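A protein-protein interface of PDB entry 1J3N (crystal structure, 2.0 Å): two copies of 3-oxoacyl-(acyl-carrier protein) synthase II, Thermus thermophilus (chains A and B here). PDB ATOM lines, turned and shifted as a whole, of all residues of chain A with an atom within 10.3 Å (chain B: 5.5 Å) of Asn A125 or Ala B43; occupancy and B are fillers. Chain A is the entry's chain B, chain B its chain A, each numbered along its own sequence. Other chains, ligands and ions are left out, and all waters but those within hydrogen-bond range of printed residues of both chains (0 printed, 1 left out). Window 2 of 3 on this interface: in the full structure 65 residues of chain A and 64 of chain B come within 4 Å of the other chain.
No position is printed for both chains. Of the 10 pairs that touch across the chains among the printed residues, none has its exchanged pair printed and touching as well.
Pro A124 touches Leu B44 (CG to CD2, 3.4 Å). Pro A124 touches Gly B198. Val B202 touches Pro A124. Asn A125 touches Leu B44 (OD1 to CD2, 3.5 Å). Asn A125 touches Pro B45 (OD1 to CD, 3.3 Å). Val B202 touches Asn A125. O of Ile A127 touches CG2 of Val B202 (3.5 Å). Val B202 touches Ser A128. Pro A129 touches Val B202 (CA to CG2, 3.96 Å).
Asn A125 touches just these residues of chain B: Ala B43, Leu B44, Pro B45 and Val B202. No residue of chain A comes within 4 Å of Ser B42. Of chain A, only Pro A124 (3.4 Å) and Asn A125 (3.5 Å) come within 4 Å of Leu B44. Of the printed residues of chain B, Pro A124 touches Leu B44 (3.4 Å), Gly B198 (3.6 Å) and Val B202 (3.9 Å). Printed residues of chain A within 4 Å of Gly B198: Pro A124. Printed residues of chain A within 4 Å of Pro B45: Asn A125 (3.3 Å). Of the printed residues of chain A, Val B202 touches Pro A124, Asn A125, Ile A127, Ser A128 and Pro A129. Printed residues of chain B within 4 Å of Ile A127: Val B202. Gln A115 touches none of the printed residues of chain B. Arg A117 touches none of the printed residues of chain B. The nearest printed residue of chain B that does not touch Ile A127 is Gly B198 (4.4 Å).
The backbone carbonyl oxygen (O) of Ala B43 sits at hydrogen-bond distance from the side-chain amide nitrogen (ND2) of Asn A125.
Printed residues of chain A that touch a printed residue of chain B: Pro A124, Asn A125, Ile A127, Ser A128 and Pro A129. Hydrophobic or aromatic side chains of chain A that line the printed part of chain B: Pro A124. Of the 9 printed residues of chain B, 5 touch a printed residue of chain A. Hydrophobic or aromatic side chains of chain B that line the printed part of chain A: Leu B44, Pro B45 and Val B202. Among the printed residues, 10 pairs touch across the chains. Among the printed residues, no Asp or Glu carboxylate lies within 4 Å of a Lys or Arg side-chain nitrogen of the other chain.
The guanidinium group of Arg B47 is in hydrogen-bond range of the backbone carbonyl oxygen of Leu B44 (2.9 Å). The side-chain amide oxygen (OE1) of Gln A115 sits at hydrogen-bond distance from the backbone NH (N) of Ser A128, 2.9 Å away.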
ATOM      1  N   GLN A 115     -13.557  23.349  30.231  1.00  0.00           N
ATOM      2  CA  GLN A 115     -14.124  23.164  28.902  1.00  0.00           C
ATOM      3  C   GLN A 115     -14.103  24.399  28.003  1.00  0.00           C
ATOM      4  O   GLN A 115     -14.040  24.276  26.780  1.00  0.00           O
ATOM      5  CB  GLN A 115     -15.542  22.604  29.015  1.00  0.00           C
ATOM      6  CG  GLN A 115     -15.575  21.170  29.533  1.00  0.00           C
ATOM      7  CD  GLN A 115     -14.723  20.237  28.689  1.00  0.00           C
ATOM      8  OE1 GLN A 115     -14.923  20.127  27.478  1.00  0.00           O
ATOM      9  NE2 GLN A 115     -13.761  19.568  29.322  1.00  0.00           N
ATOM     10  N   ARG A 117     -11.757  26.345  27.962  1.00  0.00           N
ATOM     11  CA  ARG A 117     -10.356  26.369  27.562  1.00  0.00           C
ATOM     12  C   ARG A 117     -10.159  25.395  26.400  1.00  0.00           C
ATOM     13  O   ARG A 117      -9.460  25.708  25.433  1.00  0.00           O
ATOM     14  CB  ARG A 117      -9.469  25.975  28.740  1.00  0.00           C
ATOM     15  CG  ARG A 117      -7.991  26.233  28.537  1.00  0.00           C
ATOM     16  CD  ARG A 117      -7.196  25.751  29.745  1.00  0.00           C
ATOM     17  NE  ARG A 117      -5.756  25.875  29.550  1.00  0.00           N
ATOM     18  CZ  ARG A 117      -5.092  27.027  29.543  1.00  0.00           C
ATOM     19  NH1 ARG A 117      -5.740  28.171  29.724  1.00  0.00           N
ATOM     20  NH2 ARG A 117      -3.777  27.037  29.355  1.00  0.00           N
ATOM     21  N   VAL A 118     -10.774  24.217  26.509  1.00  0.00           N
ATOM     22  CA  VAL A 118     -10.702  23.210  25.456  1.00  0.00           C
ATOM     23  C   VAL A 118     -11.295  23.827  24.196  1.00  0.00           C
ATOM     24  O   VAL A 118     -10.686  23.799  23.129  1.00  0.00           O
ATOM     25  CB  VAL A 118     -11.521  21.937  25.813  1.00  0.00           C
ATOM     26  CG1 VAL A 118     -11.674  21.049  24.581  1.00  0.00           C
ATOM     27  CG2 VAL A 118     -10.833  21.160  26.919  1.00  0.00           C
ATOM     28  N   PHE A 119     -12.487  24.397  24.329  1.00  0.00           N
ATOM     29  CA  PHE A 119     -13.167  25.028  23.208  1.00  0.00           C
ATOM     30  C   PHE A 119     -12.271  26.045  22.500  1.00  0.00           C
ATOM     31  O   PHE A 119     -12.084  25.990  21.280  1.00  0.00           O
ATOM     32  CB  PHE A 119     -14.444  25.717  23.704  1.00  0.00           C
ATOM     33  CG  PHE A 119     -15.059  26.655  22.704  1.00  0.00           C
ATOM     34  CD1 PHE A 119     -15.558  26.179  21.494  1.00  0.00           C
ATOM     35  CD2 PHE A 119     -15.115  28.023  22.963  1.00  0.00           C
ATOM     36  CE1 PHE A 119     -16.103  27.049  20.556  1.00  0.00           C
ATOM     37  CE2 PHE A 119     -15.660  28.909  22.028  1.00  0.00           C
ATOM     38  CZ  PHE A 119     -16.155  28.418  20.822  1.00  0.00           C
ATOM     39  N   LEU A 120     -11.714  26.971  23.271  1.00  0.00           N
ATOM     40  CA  LEU A 120     -10.861  28.009  22.715  1.00  0.00           C
ATOM     41  C   LEU A 120      -9.538  27.519  22.135  1.00  0.00           C
ATOM     42  O   LEU A 120      -9.077  28.030  21.116  1.00  0.00           O
ATOM     43  CB  LEU A 120     -10.600  29.084  23.776  1.00  0.00           C
ATOM     44  CG  LEU A 120     -11.806  29.973  24.085  1.00  0.00           C
ATOM     45  CD1 LEU A 120     -11.488  30.910  25.239  1.00  0.00           C
ATOM     46  CD2 LEU A 120     -12.183  30.760  22.842  1.00  0.00           C
ATOM     47  N   GLU A 121      -8.934  26.522  22.768  1.00  0.00           N
ATOM     48  CA  GLU A 121      -7.648  26.002  22.312  1.00  0.00           C
ATOM     49  C   GLU A 121      -7.706  24.824  21.353  1.00  0.00           C
ATOM     50  O   GLU A 121      -6.766  24.603  20.583  1.00  0.00           O
ATOM     51  CB  GLU A 121      -6.801  25.599  23.514  1.00  0.00           C
ATOM     52  CG  GLU A 121      -6.257  26.758  24.321  1.00  0.00           C
ATOM     53  CD  GLU A 121      -5.609  26.286  25.604  1.00  0.00           C
ATOM     54  OE1 GLU A 121      -5.090  25.149  25.611  1.00  0.00           O
ATOM     55  OE2 GLU A 121      -5.611  27.048  26.597  1.00  0.00           O
ATOM     56  N   ARG A 122      -8.793  24.061  21.392  1.00  0.00           N
ATOM     57  CA  ARG A 122      -8.896  22.894  20.529  1.00  0.00           C
ATOM     58  C   ARG A 122     -10.081  22.898  19.568  1.00  0.00           C
ATOM     59  O   ARG A 122     -10.135  22.089  18.641  1.00  0.00           O
ATOM     60  CB  ARG A 122      -8.928  21.629  21.387  1.00  0.00           C
ATOM     61  CG  ARG A 122      -7.816  21.577  22.424  1.00  0.00           C
ATOM     62  CD  ARG A 122      -7.669  20.188  23.028  1.00  0.00           C
ATOM     63  NE  ARG A 122      -6.756  20.169  24.172  1.00  0.00           N
ATOM     64  CZ  ARG A 122      -5.526  20.685  24.175  1.00  0.00           C
ATOM     65  NH1 ARG A 122      -5.042  21.275  23.090  1.00  0.00           N
ATOM     66  NH2 ARG A 122      -4.775  20.608  25.266  1.00  0.00           N
ATOM     67  N   GLY A 123     -11.027  23.808  19.783  1.00  0.00           N
ATOM     68  CA  GLY A 123     -12.184  23.874  18.911  1.00  0.00           C
ATOM     69  C   GLY A 123     -13.427  23.246  19.522  1.00  0.00           C
ATOM     70  O   GLY A 123     -13.324  22.386  20.396  1.00  0.00           O
ATOM     71  N   PRO A 124     -14.622  23.657  19.071  1.00  0.00           N
ATOM     72  CA  PRO A 124     -15.909  23.152  19.557  1.00  0.00           C
ATOM     73  C   PRO A 124     -16.170  21.668  19.317  1.00  0.00           C
ATOM     74  O   PRO A 124     -17.151  21.126  19.825  1.00  0.00           O
ATOM     75  CB  PRO A 124     -16.921  24.037  18.833  1.00  0.00           C
ATOM     76  CG  PRO A 124     -16.225  24.358  17.548  1.00  0.00           C
ATOM     77  CD  PRO A 124     -14.824  24.664  18.015  1.00  0.00           C
ATOM     78  N   ASN A 125     -15.312  21.003  18.546  1.00  0.00           N
ATOM     79  CA  ASN A 125     -15.515  19.577  18.297  1.00  0.00           C
ATOM     80  C   ASN A 125     -14.638  18.745  19.228  1.00  0.00           C
ATOM     81  O   ASN A 125     -14.672  17.513  19.189  1.00  0.00           O
ATOM     82  CB  ASN A 125     -15.210  19.218  16.841  1.00  0.00           C
ATOM     83  CG  ASN A 125     -16.088  19.968  15.849  1.00  0.00           C
ATOM     84  OD1 ASN A 125     -17.304  20.028  15.997  1.00  0.00           O
ATOM     85  ND2 ASN A 125     -15.467  20.532  14.824  1.00  0.00           N
ATOM     86  N   ARG A 126     -13.857  19.425  20.069  1.00  0.00           N
ATOM     87  CA  ARG A 126     -12.982  18.753  21.025  1.00  0.00           C
ATOM     88  C   ARG A 126     -13.638  18.778  22.405  1.00  0.00           C
ATOM     89  O   ARG A 126     -13.160  18.144  23.342  1.00  0.00           O
ATOM     90  CB  ARG A 126     -11.622  19.454  21.108  1.00  0.00           C
ATOM     91  CG  ARG A 126     -10.795  19.430  19.831  1.00  0.00           C
ATOM     92  CD  ARG A 126     -10.120  18.089  19.599  1.00  0.00           C
ATOM     93  NE  ARG A 126     -10.985  17.127  18.926  1.00  0.00           N
ATOM     94  CZ  ARG A 126     -10.579  15.933  18.502  1.00  0.00           C
ATOM     95  NH1 ARG A 126      -9.319  15.560  18.688  1.00  0.00           N
ATOM     96  NH2 ARG A 126     -11.427  15.117  17.888  1.00  0.00           N
ATOM     97  N   ILE A 127     -14.730  19.526  22.520  1.00  0.00           N
ATOM     98  CA  ILE A 127     -15.478  19.641  23.771  1.00  0.00           C
ATOM     99  C   ILE A 127     -15.912  18.268  24.296  1.00  0.00           C
ATOM    100  O   ILE A 127     -16.318  17.400  23.521  1.00  0.00           O
ATOM    101  CB  ILE A 127     -16.734  20.520  23.566  1.00  0.00           C
ATOM    102  CG1 ILE A 127     -16.305  21.938  23.176  1.00  0.00           C
ATOM    103  CG2 ILE A 127     -17.598  20.520  24.825  1.00  0.00           C
ATOM    104  CD1 ILE A 127     -17.464  22.861  22.876  1.00  0.00           C
ATOM    105  N   SER A 128     -15.821  18.079  25.613  1.00  0.00           N
ATOM    106  CA  SER A 128     -16.207  16.817  26.247  1.00  0.00           C
ATOM    107  C   SER A 128     -17.695  16.543  26.167  1.00  0.00           C
ATOM    108  O   SER A 128     -18.513  17.442  26.364  1.00  0.00           O
ATOM    109  CB  SER A 128     -15.815  16.806  27.725  1.00  0.00           C
ATOM    110  OG  SER A 128     -16.480  15.744  28.402  1.00  0.00           O
ATOM    111  N   PRO A 129     -18.073  15.285  25.894  1.00  0.00           N
ATOM    112  CA  PRO A 129     -19.503  14.982  25.818  1.00  0.00           C
ATOM    113  C   PRO A 129     -20.168  15.132  27.186  1.00  0.00           C
ATOM    114  O   PRO A 129     -21.394  15.134  27.292  1.00  0.00           O
ATOM    115  CB  PRO A 129     -19.524  13.544  25.303  1.00  0.00           C
ATOM    116  CG  PRO A 129     -18.263  12.971  25.870  1.00  0.00           C
ATOM    117  CD  PRO A 129     -17.262  14.083  25.635  1.00  0.00           C
ATOM    118  N   ASP B  40     -20.403  31.642  12.189  1.00  0.00           N
ATOM    119  CA  ASP B  40     -19.962  30.700  11.170  1.00  0.00           C
ATOM    120  C   ASP B  40     -19.820  29.300  11.758  1.00  0.00           C
ATOM    121  O   ASP B  40     -18.861  28.996  12.471  1.00  0.00           O
ATOM    122  CB  ASP B  40     -18.636  31.155  10.564  1.00  0.00           C
ATOM    123  CG  ASP B  40     -18.026  30.112   9.646  1.00  0.00           C
ATOM    124  OD1 ASP B  40     -18.766  29.218   9.180  1.00  0.00           O
ATOM    125  OD2 ASP B  40     -16.806  30.192   9.385  1.00  0.00           O
ATOM    126  N   ALA B  41     -20.783  28.444  11.451  1.00  0.00           N
ATOM    127  CA  ALA B  41     -20.768  27.082  11.962  1.00  0.00           C
ATOM    128  C   ALA B  41     -20.282  26.082  10.908  1.00  0.00           C
ATOM    129  O   ALA B  41     -20.608  24.900  10.980  1.00  0.00           O
ATOM    130  CB  ALA B  41     -22.171  26.703  12.449  1.00  0.00           C
ATOM    131  N   SER B  42     -19.490  26.549   9.943  1.00  0.00           N
ATOM    132  CA  SER B  42     -18.995  25.664   8.886  1.00  0.00           C
ATOM    133  C   SER B  42     -18.208  24.472   9.439  1.00  0.00           C
ATOM    134  O   SER B  42     -18.412  23.345   9.011  1.00  0.00           O
ATOM    135  CB  SER B  42     -18.140  26.446   7.865  1.00  0.00           C
ATOM    136  OG  SER B  42     -16.816  26.679   8.319  1.00  0.00           O
ATOM    137  N   ALA B  43     -17.338  24.698  10.414  1.00  0.00           N
ATOM    138  CA  ALA B  43     -16.549  23.598  10.968  1.00  0.00           C
ATOM    139  C   ALA B  43     -17.341  22.564  11.784  1.00  0.00           C
ATOM    140  O   ALA B  43     -16.864  21.446  11.994  1.00  0.00           O
ATOM    141  CB  ALA B  43     -15.407  24.158  11.813  1.00  0.00           C
ATOM    142  N   LEU B  44     -18.541  22.926  12.238  1.00  0.00           N
ATOM    143  CA  LEU B  44     -19.362  22.017  13.047  1.00  0.00           C
ATOM    144  C   LEU B  44     -20.131  20.954  12.257  1.00  0.00           C
ATOM    145  O   LEU B  44     -20.368  21.107  11.061  1.00  0.00           O
ATOM    146  CB  LEU B  44     -20.366  22.817  13.881  1.00  0.00           C
ATOM    147  CG  LEU B  44     -19.840  23.825  14.906  1.00  0.00           C
ATOM    148  CD1 LEU B  44     -21.019  24.448  15.647  1.00  0.00           C
ATOM    149  CD2 LEU B  44     -18.911  23.135  15.879  1.00  0.00           C
ATOM    150  N   PRO B  45     -20.517  19.849  12.929  1.00  0.00           N
ATOM    151  CA  PRO B  45     -21.271  18.757  12.296  1.00  0.00           C
ATOM    152  C   PRO B  45     -22.752  19.106  12.182  1.00  0.00           C
ATOM    153  O   PRO B  45     -23.479  18.531  11.366  1.00  0.00           O
ATOM    154  CB  PRO B  45     -21.026  17.577  13.236  1.00  0.00           C
ATOM    155  CG  PRO B  45     -20.901  18.231  14.570  1.00  0.00           C
ATOM    156  CD  PRO B  45     -20.011  19.426  14.249  1.00  0.00           C
ATOM    157  N   ARG B  47     -25.093  22.334  11.524  1.00  0.00           N
ATOM    158  CA  ARG B  47     -24.993  23.700  11.029  1.00  0.00           C
ATOM    159  C   ARG B  47     -26.334  24.366  10.760  1.00  0.00           C
ATOM    160  O   ARG B  47     -26.432  25.262   9.910  1.00  0.00           O
ATOM    161  CB  ARG B  47     -24.126  23.691   9.762  1.00  0.00           C
ATOM    162  CG  ARG B  47     -22.791  22.975   9.978  1.00  0.00           C
ATOM    163  CD  ARG B  47     -21.914  22.975   8.733  1.00  0.00           C
ATOM    164  NE  ARG B  47     -22.407  22.084   7.681  1.00  0.00           N
ATOM    165  CZ  ARG B  47     -22.176  20.776   7.629  1.00  0.00           C
ATOM    166  NH1 ARG B  47     -21.451  20.186   8.572  1.00  0.00           N
ATOM    167  NH2 ARG B  47     -22.662  20.058   6.622  1.00  0.00           N
ATOM    168  N   GLY B 198     -21.718  22.991  19.722  1.00  0.00           N
ATOM    169  CA  GLY B 198     -20.607  22.059  19.649  1.00  0.00           C
ATOM    170  C   GLY B 198     -20.758  20.990  20.717  1.00  0.00           C
ATOM    171  O   GLY B 198     -20.602  19.797  20.450  1.00  0.00           O
ATOM    172  N   VAL B 202     -21.221  17.022  20.070  1.00  0.00           N
ATOM    173  CA  VAL B 202     -20.318  15.958  20.502  1.00  0.00           C
ATOM    174  C   VAL B 202     -21.084  14.930  21.341  1.00  0.00           C
ATOM    175  O   VAL B 202     -20.654  13.786  21.471  1.00  0.00           O
ATOM    176  CB  VAL B 202     -19.129  16.499  21.326  1.00  0.00           C
ATOM    177  CG1 VAL B 202     -18.287  17.425  20.465  1.00  0.00           C
ATOM    178  CG2 VAL B 202     -19.636  17.229  22.566  1.00  0.00           C
